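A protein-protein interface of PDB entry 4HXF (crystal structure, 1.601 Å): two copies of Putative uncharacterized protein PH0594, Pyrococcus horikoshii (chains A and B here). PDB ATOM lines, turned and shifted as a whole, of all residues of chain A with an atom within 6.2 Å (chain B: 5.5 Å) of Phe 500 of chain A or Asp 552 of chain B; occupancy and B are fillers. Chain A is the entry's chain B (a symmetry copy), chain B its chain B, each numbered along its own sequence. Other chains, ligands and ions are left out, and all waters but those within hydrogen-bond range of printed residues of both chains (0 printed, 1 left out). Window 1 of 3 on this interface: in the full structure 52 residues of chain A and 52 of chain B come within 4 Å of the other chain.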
ATOM      1  N   TRP A 140      32.403  28.915  19.330  1.00  0.00           N
ATOM      2  CA  TRP A 140      32.989  28.631  20.659  1.00  0.00           C
ATOM      3  C   TRP A 140      34.445  28.308  20.582  1.00  0.00           C
ATOM      4  O   TRP A 140      35.007  28.092  19.489  1.00  0.00           O
ATOM      5  CB  TRP A 140      32.143  27.508  21.314  1.00  0.00           C
ATOM      6  CG  TRP A 140      32.136  26.141  20.604  1.00  0.00           C
ATOM      7  CD1 TRP A 140      32.860  25.728  19.551  1.00  0.00           C
ATOM      8  CD2 TRP A 140      31.246  25.068  20.992  1.00  0.00           C
ATOM      9  NE1 TRP A 140      32.485  24.405  19.182  1.00  0.00           N
ATOM     10  CE2 TRP A 140      31.503  23.948  20.081  1.00  0.00           C
ATOM     11  CE3 TRP A 140      30.285  24.923  22.002  1.00  0.00           C
ATOM     12  CZ2 TRP A 140      30.808  22.732  20.215  1.00  0.00           C
ATOM     13  CZ3 TRP A 140      29.588  23.740  22.097  1.00  0.00           C
ATOM     14  CH2 TRP A 140      29.874  22.667  21.242  1.00  0.00           C
ATOM     15  N   LEU A 495      34.529  13.750  10.800  1.00  0.00           N
ATOM     16  CA  LEU A 495      33.697  14.706  10.122  1.00  0.00           C
ATOM     17  C   LEU A 495      33.034  15.641  11.120  1.00  0.00           C
ATOM     18  O   LEU A 495      32.948  16.859  10.898  1.00  0.00           O
ATOM     19  CB  LEU A 495      32.584  14.068   9.270  1.00  0.00           C
ATOM     20  CG  LEU A 495      31.851  15.023   8.350  1.00  0.00           C
ATOM     21  CD1 LEU A 495      32.723  15.707   7.310  1.00  0.00           C
ATOM     22  CD2 LEU A 495      30.731  14.382   7.571  1.00  0.00           C
ATOM     23  N   THR A 496      32.595  15.121  12.291  1.00  0.00           N
ATOM     24  CA  THR A 496      32.054  16.008  13.314  1.00  0.00           C
ATOM     25  C   THR A 496      33.101  16.874  13.986  1.00  0.00           C
ATOM     26  O   THR A 496      32.814  17.939  14.533  1.00  0.00           O
ATOM     27  CB  THR A 496      31.164  15.267  14.332  1.00  0.00           C
ATOM     28  OG1 THR A 496      31.985  14.367  15.061  1.00  0.00           O
ATOM     29  CG2 THR A 496      30.037  14.548  13.568  1.00  0.00           C
ATOM     30  N   SER A 497      34.367  16.391  14.062  1.00  0.00           N
ATOM     31  CA  SER A 497      35.419  17.262  14.503  1.00  0.00           C
ATOM     32  C   SER A 497      35.525  18.478  13.577  1.00  0.00           C
ATOM     33  O   SER A 497      35.570  19.631  14.003  1.00  0.00           O
ATOM     34  CB  SER A 497      36.740  16.465  14.549  1.00  0.00           C
ATOM     35  OG  SER A 497      37.869  17.354  14.840  1.00  0.00           O
ATOM     36  N   TYR A 498      35.611  18.237  12.272  1.00  0.00           N
ATOM     37  CA  TYR A 498      35.610  19.342  11.286  1.00  0.00           C
ATOM     38  C   TYR A 498      34.555  20.404  11.533  1.00  0.00           C
ATOM     39  O   TYR A 498      34.768  21.578  11.573  1.00  0.00           O
ATOM     40  CB  TYR A 498      35.551  18.785   9.853  1.00  0.00           C
ATOM     41  CG  TYR A 498      35.111  19.795   8.807  1.00  0.00           C
ATOM     42  CD1 TYR A 498      35.880  20.933   8.490  1.00  0.00           C
ATOM     43  CD2 TYR A 498      33.918  19.666   8.194  1.00  0.00           C
ATOM     44  CE1 TYR A 498      35.446  21.820   7.596  1.00  0.00           C
ATOM     45  CE2 TYR A 498      33.486  20.575   7.263  1.00  0.00           C
ATOM     46  CZ  TYR A 498      34.200  21.659   6.985  1.00  0.00           C
ATOM     47  OH  TYR A 498      33.720  22.567   6.070  1.00  0.00           O
ATOM     48  N   ALA A 499      33.273  19.894  11.624  1.00  0.00           N
ATOM     49  CA  ALA A 499      32.141  20.771  11.606  1.00  0.00           C
ATOM     50  C   ALA A 499      31.661  21.313  12.973  1.00  0.00           C
ATOM     51  O   ALA A 499      31.020  22.341  12.965  1.00  0.00           O
ATOM     52  CB  ALA A 499      30.938  20.086  10.874  1.00  0.00           C
ATOM     53  N   PHE A 500      31.986  20.626  14.048  1.00  0.00           N
ATOM     54  CA  PHE A 500      31.561  21.005  15.399  1.00  0.00           C
ATOM     55  C   PHE A 500      32.593  21.608  16.289  1.00  0.00           C
ATOM     56  O   PHE A 500      32.242  22.416  17.162  1.00  0.00           O
ATOM     57  CB  PHE A 500      30.938  19.741  16.006  1.00  0.00           C
ATOM     58  CG  PHE A 500      29.985  19.958  17.199  1.00  0.00           C
ATOM     59  CD1 PHE A 500      29.097  21.005  17.266  1.00  0.00           C
ATOM     60  CD2 PHE A 500      29.872  18.933  18.158  1.00  0.00           C
ATOM     61  CE1 PHE A 500      28.203  21.082  18.330  1.00  0.00           C
ATOM     62  CE2 PHE A 500      28.955  19.010  19.201  1.00  0.00           C
ATOM     63  CZ  PHE A 500      28.161  20.129  19.332  1.00  0.00           C
ATOM     64  N   SER A 501      33.862  21.218  16.171  1.00  0.00           N
ATOM     65  CA  SER A 501      34.875  21.697  17.096  1.00  0.00           C
ATOM     66  C   SER A 501      35.311  23.110  16.844  1.00  0.00           C
ATOM     67  O   SER A 501      35.069  23.691  15.815  1.00  0.00           O
ATOM     68  CB  SER A 501      36.078  20.820  17.118  1.00  0.00           C
ATOM     69  OG  SER A 501      36.848  20.985  15.936  1.00  0.00           O
ATOM     70  N   ASP A 502      35.950  23.670  17.844  1.00  0.00           N
ATOM     71  CA  ASP A 502      36.406  25.040  17.725  1.00  0.00           C
ATOM     72  C   ASP A 502      37.347  25.309  16.561  1.00  0.00           C
ATOM     73  O   ASP A 502      37.258  26.384  15.937  1.00  0.00           O
ATOM     74  CB  ASP A 502      36.956  25.517  19.051  1.00  0.00           C
ATOM     75  CG  ASP A 502      38.157  24.734  19.574  1.00  0.00           C
ATOM     76  OD1 ASP A 502      38.598  23.769  19.023  1.00  0.00           O
ATOM     77  OD2 ASP A 502      38.605  25.169  20.633  1.00  0.00           O
ATOM     78  N   GLY A 504      38.045  22.989  14.044  1.00  0.00           N
ATOM     79  CA  GLY A 504      37.929  22.047  12.995  1.00  0.00           C
ATOM     80  C   GLY A 504      37.858  22.531  11.609  1.00  0.00           C
ATOM     81  O   GLY A 504      38.328  21.853  10.717  1.00  0.00           O
ATOM     82  N   TYR A 547      35.528  22.111  24.017  1.00  0.00           N
ATOM     83  CA  TYR A 547      35.113  22.498  22.655  1.00  0.00           C
ATOM     84  C   TYR A 547      36.127  22.143  21.581  1.00  0.00           C
ATOM     85  O   TYR A 547      35.872  22.334  20.369  1.00  0.00           O
ATOM     86  CB  TYR A 547      34.719  23.953  22.597  1.00  0.00           C
ATOM     87  CG  TYR A 547      33.688  24.299  23.704  1.00  0.00           C
ATOM     88  CD1 TYR A 547      33.868  25.413  24.504  1.00  0.00           C
ATOM     89  CD2 TYR A 547      32.626  23.470  23.953  1.00  0.00           C
ATOM     90  CE1 TYR A 547      32.975  25.676  25.516  1.00  0.00           C
ATOM     91  CE2 TYR A 547      31.720  23.751  25.006  1.00  0.00           C
ATOM     92  CZ  TYR A 547      31.926  24.872  25.763  1.00  0.00           C
ATOM     93  OH  TYR A 547      31.074  25.180  26.848  1.00  0.00           O
ATOM     94  N   PRO A 550      34.528  18.039  21.062  1.00  0.00           N
ATOM     95  CA  PRO A 550      33.238  18.071  21.731  1.00  0.00           C
ATOM     96  C   PRO A 550      32.709  16.698  22.114  1.00  0.00           C
ATOM     97  O   PRO A 550      33.209  15.664  21.738  1.00  0.00           O
ATOM     98  CB  PRO A 550      32.313  18.773  20.722  1.00  0.00           C
ATOM     99  CG  PRO A 550      33.238  19.572  19.828  1.00  0.00           C
ATOM    100  CD  PRO A 550      34.475  18.741  19.734  1.00  0.00           C
ATOM    101  N   LEU A 551      31.688  16.780  22.980  1.00  0.00           N
ATOM    102  CA  LEU A 551      31.062  15.570  23.627  1.00  0.00           C
ATOM    103  C   LEU A 551      30.724  14.436  22.698  1.00  0.00           C
ATOM    104  O   LEU A 551      30.851  13.276  23.076  1.00  0.00           O
ATOM    105  CB  LEU A 551      29.887  16.019  24.441  1.00  0.00           C
ATOM    106  CG  LEU A 551      29.208  14.832  25.236  1.00  0.00           C
ATOM    107  CD1 LEU A 551      30.123  14.161  26.288  1.00  0.00           C
ATOM    108  CD2 LEU A 551      27.869  15.390  25.875  1.00  0.00           C
ATOM    109  N   ASP A 552      30.219  14.750  21.503  1.00  0.00           N
ATOM    110  CA  ASP A 552      29.818  13.775  20.514  1.00  0.00           C
ATOM    111  C   ASP A 552      30.938  12.755  20.274  1.00  0.00           C
ATOM    112  O   ASP A 552      30.710  11.566  20.062  1.00  0.00           O
ATOM    113  CB  ASP A 552      29.334  14.391  19.195  1.00  0.00           C
ATOM    114  CG  ASP A 552      30.428  15.102  18.456  1.00  0.00           C
ATOM    115  OD1 ASP A 552      30.577  14.788  17.271  1.00  0.00           O
ATOM    116  OD2 ASP A 552      31.110  15.977  19.081  1.00  0.00           O
ATOM    117  N   MET A 556      29.023   9.489  21.076  1.00  0.00           N
ATOM    118  CA  MET A 556      28.623   8.711  19.896  1.00  0.00           C
ATOM    119  C   MET A 556      29.277   7.349  19.935  1.00  0.00           C
ATOM    120  O   MET A 556      28.637   6.382  19.620  1.00  0.00           O
ATOM    121  CB  MET A 556      28.860   9.440  18.559  1.00  0.00           C
ATOM    122  CG  MET A 556      28.098  10.680  18.344  1.00  0.00           C
ATOM    123  SD  MET A 556      28.278  11.311  16.639  1.00  0.00           S
ATOM    124  CE  MET A 556      30.026  11.548  16.505  1.00  0.00           C
ATOM    125  N   SER B 492      20.503  18.299  10.480  1.00  0.00           N
ATOM    126  CA  SER B 492      21.386  18.467   9.334  1.00  0.00           C
ATOM    127  C   SER B 492      22.147  17.181   8.936  1.00  0.00           C
ATOM    128  O   SER B 492      22.521  17.117   7.761  1.00  0.00           O
ATOM    129  CB  SER B 492      22.394  19.638   9.415  1.00  0.00           C
ATOM    130  OG  SER B 492      23.331  19.474  10.450  1.00  0.00           O
ATOM    131  N   THR B 496      24.832  11.580  12.972  1.00  0.00           N
ATOM    132  CA  THR B 496      24.969  12.040  14.349  1.00  0.00           C
ATOM    133  C   THR B 496      23.677  11.994  15.139  1.00  0.00           C
ATOM    134  O   THR B 496      23.665  11.926  16.368  1.00  0.00           O
ATOM    135  CB  THR B 496      25.671  13.409  14.450  1.00  0.00           C
ATOM    136  OG1 THR B 496      24.828  14.381  13.850  1.00  0.00           O
ATOM    137  CG2 THR B 496      27.043  13.311  13.758  1.00  0.00           C
ATOM    138  N   SER B 497      22.512  12.136  14.455  1.00  0.00           N
ATOM    139  CA  SER B 497      21.273  11.894  15.135  1.00  0.00           C
ATOM    140  C   SER B 497      21.232  10.459  15.672  1.00  0.00           C
ATOM    141  O   SER B 497      20.919  10.197  16.832  1.00  0.00           O
ATOM    142  CB  SER B 497      20.108  12.170  14.161  1.00  0.00           C
ATOM    143  OG  SER B 497      18.828  11.782  14.763  1.00  0.00           O
ATOM    144  N   PHE B 500      24.201  10.210  18.583  1.00  0.00           N
ATOM    145  CA  PHE B 500      24.217  11.197  19.667  1.00  0.00           C
ATOM    146  C   PHE B 500      22.921  11.476  20.347  1.00  0.00           C
ATOM    147  O   PHE B 500      22.925  11.825  21.537  1.00  0.00           O
ATOM    148  CB  PHE B 500      24.839  12.463  19.065  1.00  0.00           C
ATOM    149  CG  PHE B 500      25.423  13.478  20.067  1.00  0.00           C
ATOM    150  CD1 PHE B 500      26.110  13.103  21.197  1.00  0.00           C
ATOM    151  CD2 PHE B 500      25.435  14.840  19.708  1.00  0.00           C
ATOM    152  CE1 PHE B 500      26.689  14.076  22.006  1.00  0.00           C
ATOM    153  CE2 PHE B 500      26.042  15.799  20.511  1.00  0.00           C
ATOM    154  CZ  PHE B 500      26.612  15.427  21.711  1.00  0.00           C
ATOM    155  N   HIS B 542      18.680  27.010  18.238  1.00  0.00           N
ATOM    156  CA  HIS B 542      18.888  25.781  18.981  1.00  0.00           C
ATOM    157  C   HIS B 542      18.885  26.081  20.458  1.00  0.00           C
ATOM    158  O   HIS B 542      18.833  27.224  20.868  1.00  0.00           O
ATOM    159  CB  HIS B 542      20.184  25.095  18.610  1.00  0.00           C
ATOM    160  CG  HIS B 542      20.052  23.585  18.606  1.00  0.00           C
ATOM    161  ND1 HIS B 542      19.713  22.876  17.450  1.00  0.00           N
ATOM    162  CD2 HIS B 542      20.142  22.638  19.652  1.00  0.00           C
ATOM    163  CE1 HIS B 542      19.650  21.568  17.775  1.00  0.00           C
ATOM    164  NE2 HIS B 542      19.824  21.414  19.089  1.00  0.00           N
ATOM    165  N   CYS B 549      17.334  16.474  19.414  1.00  0.00           N
ATOM    166  CA  CYS B 549      18.145  16.951  18.313  1.00  0.00           C
ATOM    167  C   CYS B 549      19.264  17.757  18.977  1.00  0.00           C
ATOM    168  O   CYS B 549      19.123  18.982  19.222  1.00  0.00           O
ATOM    169  CB  CYS B 549      17.396  17.803  17.321  1.00  0.00           C
ATOM    170  SG  CYS B 549      16.027  16.899  16.495  1.00  0.00           S
ATOM    171  N   PRO B 550      20.374  17.086  19.215  1.00  0.00           N
ATOM    172  CA  PRO B 550      21.437  17.810  19.892  1.00  0.00           C
ATOM    173  C   PRO B 550      22.040  18.934  19.065  1.00  0.00           C
ATOM    174  O   PRO B 550      21.801  19.099  17.891  1.00  0.00           O
ATOM    175  CB  PRO B 550      22.477  16.725  20.217  1.00  0.00           C
ATOM    176  CG  PRO B 550      21.703  15.423  20.216  1.00  0.00           C
ATOM    177  CD  PRO B 550      20.659  15.612  19.166  1.00  0.00           C
ATOM    178  N   LEU B 551      22.790  19.758  19.812  1.00  0.00           N
ATOM    179  CA  LEU B 551      23.398  21.029  19.275  1.00  0.00           C
ATOM    180  C   LEU B 551      24.114  20.902  17.957  1.00  0.00           C
ATOM    181  O   LEU B 551      24.060  21.817  17.141  1.00  0.00           O
ATOM    182  CB  LEU B 551      24.257  21.635  20.342  1.00  0.00           C
ATOM    183  CG  LEU B 551      24.875  23.025  19.910  1.00  0.00           C
ATOM    184  CD1 LEU B 551      23.829  24.132  19.634  1.00  0.00           C
ATOM    185  CD2 LEU B 551      25.918  23.451  21.023  1.00  0.00           C
ATOM    186  N   ASP B 552      24.853  19.808  17.762  1.00  0.00           N
ATOM    187  CA  ASP B 552      25.622  19.556  16.564  1.00  0.00           C
ATOM    188  C   ASP B 552      24.752  19.740  15.314  1.00  0.00           C
ATOM    189  O   ASP B 552      25.191  20.226  14.275  1.00  0.00           O
ATOM    190  CB  ASP B 552      26.329  18.195  16.555  1.00  0.00           C
ATOM    191  CG  ASP B 552      25.366  17.046  16.514  1.00  0.00           C
ATOM    192  OD1 ASP B 552      25.564  16.201  15.635  1.00  0.00           O
ATOM    193  OD2 ASP B 552      24.433  17.007  17.380  1.00  0.00           O
ATOM    194  N   GLN B 553      23.491  19.383  15.447  1.00  0.00           N
ATOM    195  CA  GLN B 553      22.613  19.430  14.275  1.00  0.00           C
ATOM    196  C   GLN B 553      22.472  20.844  13.710  1.00  0.00           C
ATOM    197  O   GLN B 553      22.364  21.011  12.506  1.00  0.00           O
ATOM    198  CB  GLN B 553      21.211  18.898  14.568  1.00  0.00           C
ATOM    199  CG  GLN B 553      21.127  17.409  14.921  1.00  0.00           C
ATOM    200  CD  GLN B 553      21.710  16.534  13.802  1.00  0.00           C
ATOM    201  OE1 GLN B 553      21.718  16.989  12.638  1.00  0.00           O
ATOM    202  NE2 GLN B 553      22.235  15.316  14.129  1.00  0.00           N
ATOM    203  N   SER B 554      22.456  21.835  14.555  1.00  0.00           N
ATOM    204  CA  SER B 554      22.439  23.255  14.133  1.00  0.00           C
ATOM    205  C   SER B 554      23.836  23.787  13.975  1.00  0.00           C
ATOM    206  O   SER B 554      24.104  24.458  12.964  1.00  0.00           O
ATOM    207  CB  SER B 554      21.617  24.212  14.996  1.00  0.00           C
ATOM    208  OG  SER B 554      20.208  23.878  14.952  1.00  0.00           O
ATOM    209  N   LEU B 555      24.715  23.510  14.948  1.00  0.00           N
ATOM    210  CA  LEU B 555      26.026  24.205  14.926  1.00  0.00           C
ATOM    211  C   LEU B 555      26.916  23.702  13.782  1.00  0.00           C
ATOM    212  O   LEU B 555      27.662  24.480  13.122  1.00  0.00           O
ATOM    213  CB  LEU B 555      26.691  24.135  16.288  1.00  0.00           C
ATOM    214  CG  LEU B 555      28.045  24.868  16.420  1.00  0.00           C
ATOM    215  CD1 LEU B 555      27.849  26.348  15.977  1.00  0.00           C
ATOM    216  CD2 LEU B 555      28.610  24.808  17.886  1.00  0.00           C
ATOM    217  N   MET B 556      26.845  22.414  13.457  1.00  0.00           N
ATOM    218  CA  MET B 556      27.633  21.897  12.330  1.00  0.00           C
ATOM    219  C   MET B 556      27.188  22.561  11.048  1.00  0.00           C
ATOM    220  O   MET B 556      28.016  22.902  10.245  1.00  0.00           O
ATOM    221  CB  MET B 556      27.638  20.360  12.226  1.00  0.00           C
ATOM    222  CG  MET B 556      28.247  19.628  13.348  1.00  0.00           C
ATOM    223  SD  MET B 556      28.414  17.844  12.997  1.00  0.00           S
ATOM    224  CE  MET B 556      26.740  17.360  12.691  1.00  0.00           C
ATOM    225  N   PHE B 557      25.882  22.646  10.817  1.00  0.00           N
ATOM    226  CA  PHE B 557      25.298  23.252   9.651  1.00  0.00           C
ATOM    227  C   PHE B 557      25.703  24.747   9.566  1.00  0.00           C
ATOM    228  O   PHE B 557      26.181  25.207   8.510  1.00  0.00           O
ATOM    229  CB  PHE B 557      23.820  23.030   9.578  1.00  0.00           C
ATOM    230  CG  PHE B 557      23.188  23.233   8.209  1.00  0.00           C
ATOM    231  CD1 PHE B 557      23.685  22.707   7.006  1.00  0.00           C
ATOM    232  CD2 PHE B 557      21.921  23.798   8.143  1.00  0.00           C
ATOM    233  CE1 PHE B 557      23.038  22.930   5.815  1.00  0.00           C
ATOM    234  CE2 PHE B 557      21.249  23.938   6.933  1.00  0.00           C
ATOM    235  CZ  PHE B 557      21.761  23.432   5.798  1.00  0.00           C
ATOM    236  N   HIS B 559      28.459  26.178  11.052  1.00  0.00           N
ATOM    237  CA  HIS B 559      29.877  26.317  10.715  1.00  0.00           C
ATOM    238  C   HIS B 559      30.231  26.031   9.252  1.00  0.00           C
ATOM    239  O   HIS B 559      31.053  26.708   8.624  1.00  0.00           O
ATOM    240  CB  HIS B 559      30.756  25.409  11.598  1.00  0.00           C
ATOM    241  CG  HIS B 559      30.899  25.839  13.012  1.00  0.00           C
ATOM    242  ND1 HIS B 559      31.288  24.992  14.019  1.00  0.00           N
ATOM    243  CD2 HIS B 559      30.894  27.150  13.596  1.00  0.00           C
ATOM    244  CE1 HIS B 559      31.483  25.758  15.189  1.00  0.00           C
ATOM    245  NE2 HIS B 559      31.257  27.044  14.893  1.00  0.00           N
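Hydrophobic or aromatic side chains of chain A within 4 Å of the printed part of chain B: Trp 140, Ala 499, Phe 500 and Met 556.
Printed residues of chain B that touch a printed residue of chain A: Thr 496, Phe 500, Leu 551, Asp 552, Leu 555, Met 556 and His 559.
Hydrophobic or aromatic side chains of chain B that line the printed part of chain A: Phe 500, Leu 551, Leu 555, Met 556 and His 559.
Among the printed residues, 14 pairs touch across the chains.
Among the printed residues, merely in contact across the chains: Thr 496 of chain A with Thr 496 of chain B, Ala 499 of chain A with Met 556 of chain B, Asp 552 of chain A with Phe 500 of chain B, Phe 500 of chain A with Asp 552 of chain B, Thr 496 of chain A with Met 556 of chain B, Met 556 of chain A with Thr 496 of chain B, Trp 140 of chain A with Leu 555 of chain B, Phe 500 of chain A with Leu 555 of chain B, Phe 500 of chain A with Met 556 of chain B, Met 556 of chain A with Phe 500 of chain B, Trp 140 of chain A with Leu 551 of chain B, Phe 500 of chain A with His 559 of chain B and Ala 499 of chain A with Leu 555 of chain B.
The indole nitrogen of Trp 140 of chain A lies within hydrogen-bond range of the backbone carbonyl oxygen of Phe 500 of chain A.
The side-chain hydroxyl (OG1) of Thr 496 of chain B lies within hydrogen-bond range of the side-chain amide nitrogen (NE2) of Gln 553 of chain B, 2.8 Å away.
OG1 of Thr 496 of chain A is in hydrogen-bond range of OD1 of Asp 552 of chain A (2.7 Å).
The side-chain hydroxyl (OG1) of Thr 496 of chain B is in hydrogen-bond range of the side-chain carboxylate (OD1) of Asp 552 of chain B.
A ring nitrogen (NE2) of His 542 of chain B is in hydrogen-bond range of the backbone NH of Leu 551 of chain B (3.5 Å).
O of Ala 499 of chain A lies within hydrogen-bond range of ND1 of His 559 of chain B (2.9 Å).
Phe 500 of chain A touches just these residues of chain B: Asp 552 (3.5 Å), Leu 555 (3.8 Å), Met 556 (3.8 Å) and His 559 (3.95 Å).
Of chain A, only Phe 500 (3.5 Å) comes within 4 Å of Asp 552 of chain B.
Of the printed residues of chain A, Met 556 of chain B touches Thr 496, Ala 499 and Phe 500.
Of the printed residues of chain B, Met 556 of chain A touches Thr 496 and Phe 500.
Gln 553 of chain B touches none of the printed residues of chain A.
Pro 550 of chain B touches none of the printed residues of chain A.
The nearest residue of chain A that does not touch Asp 552 of chain B is Thr 496 of chain A (5.2 Å).
Thr 496 of chain B touches its own counterpart, Thr 496 of chain A.
Thr 496 of chain A touches Met 556 of chain B, and with the chains exchanged Met 556 of chain A touches Thr 496 of chain B.
Phe 500 of chain A touches Asp 552 of chain B, and with the chains exchanged Asp 552 of chain A touches Phe 500 of chain B.
Phe 500 of chain A touches Met 556 of chain B, and with the chains exchanged Met 556 of chain A touches Phe 500 of chain B.
7 positions are printed for both chains.
Of the 14 pairs that touch across the chains among the printed residues, 7 have their exchanged pair printed and touching as well.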
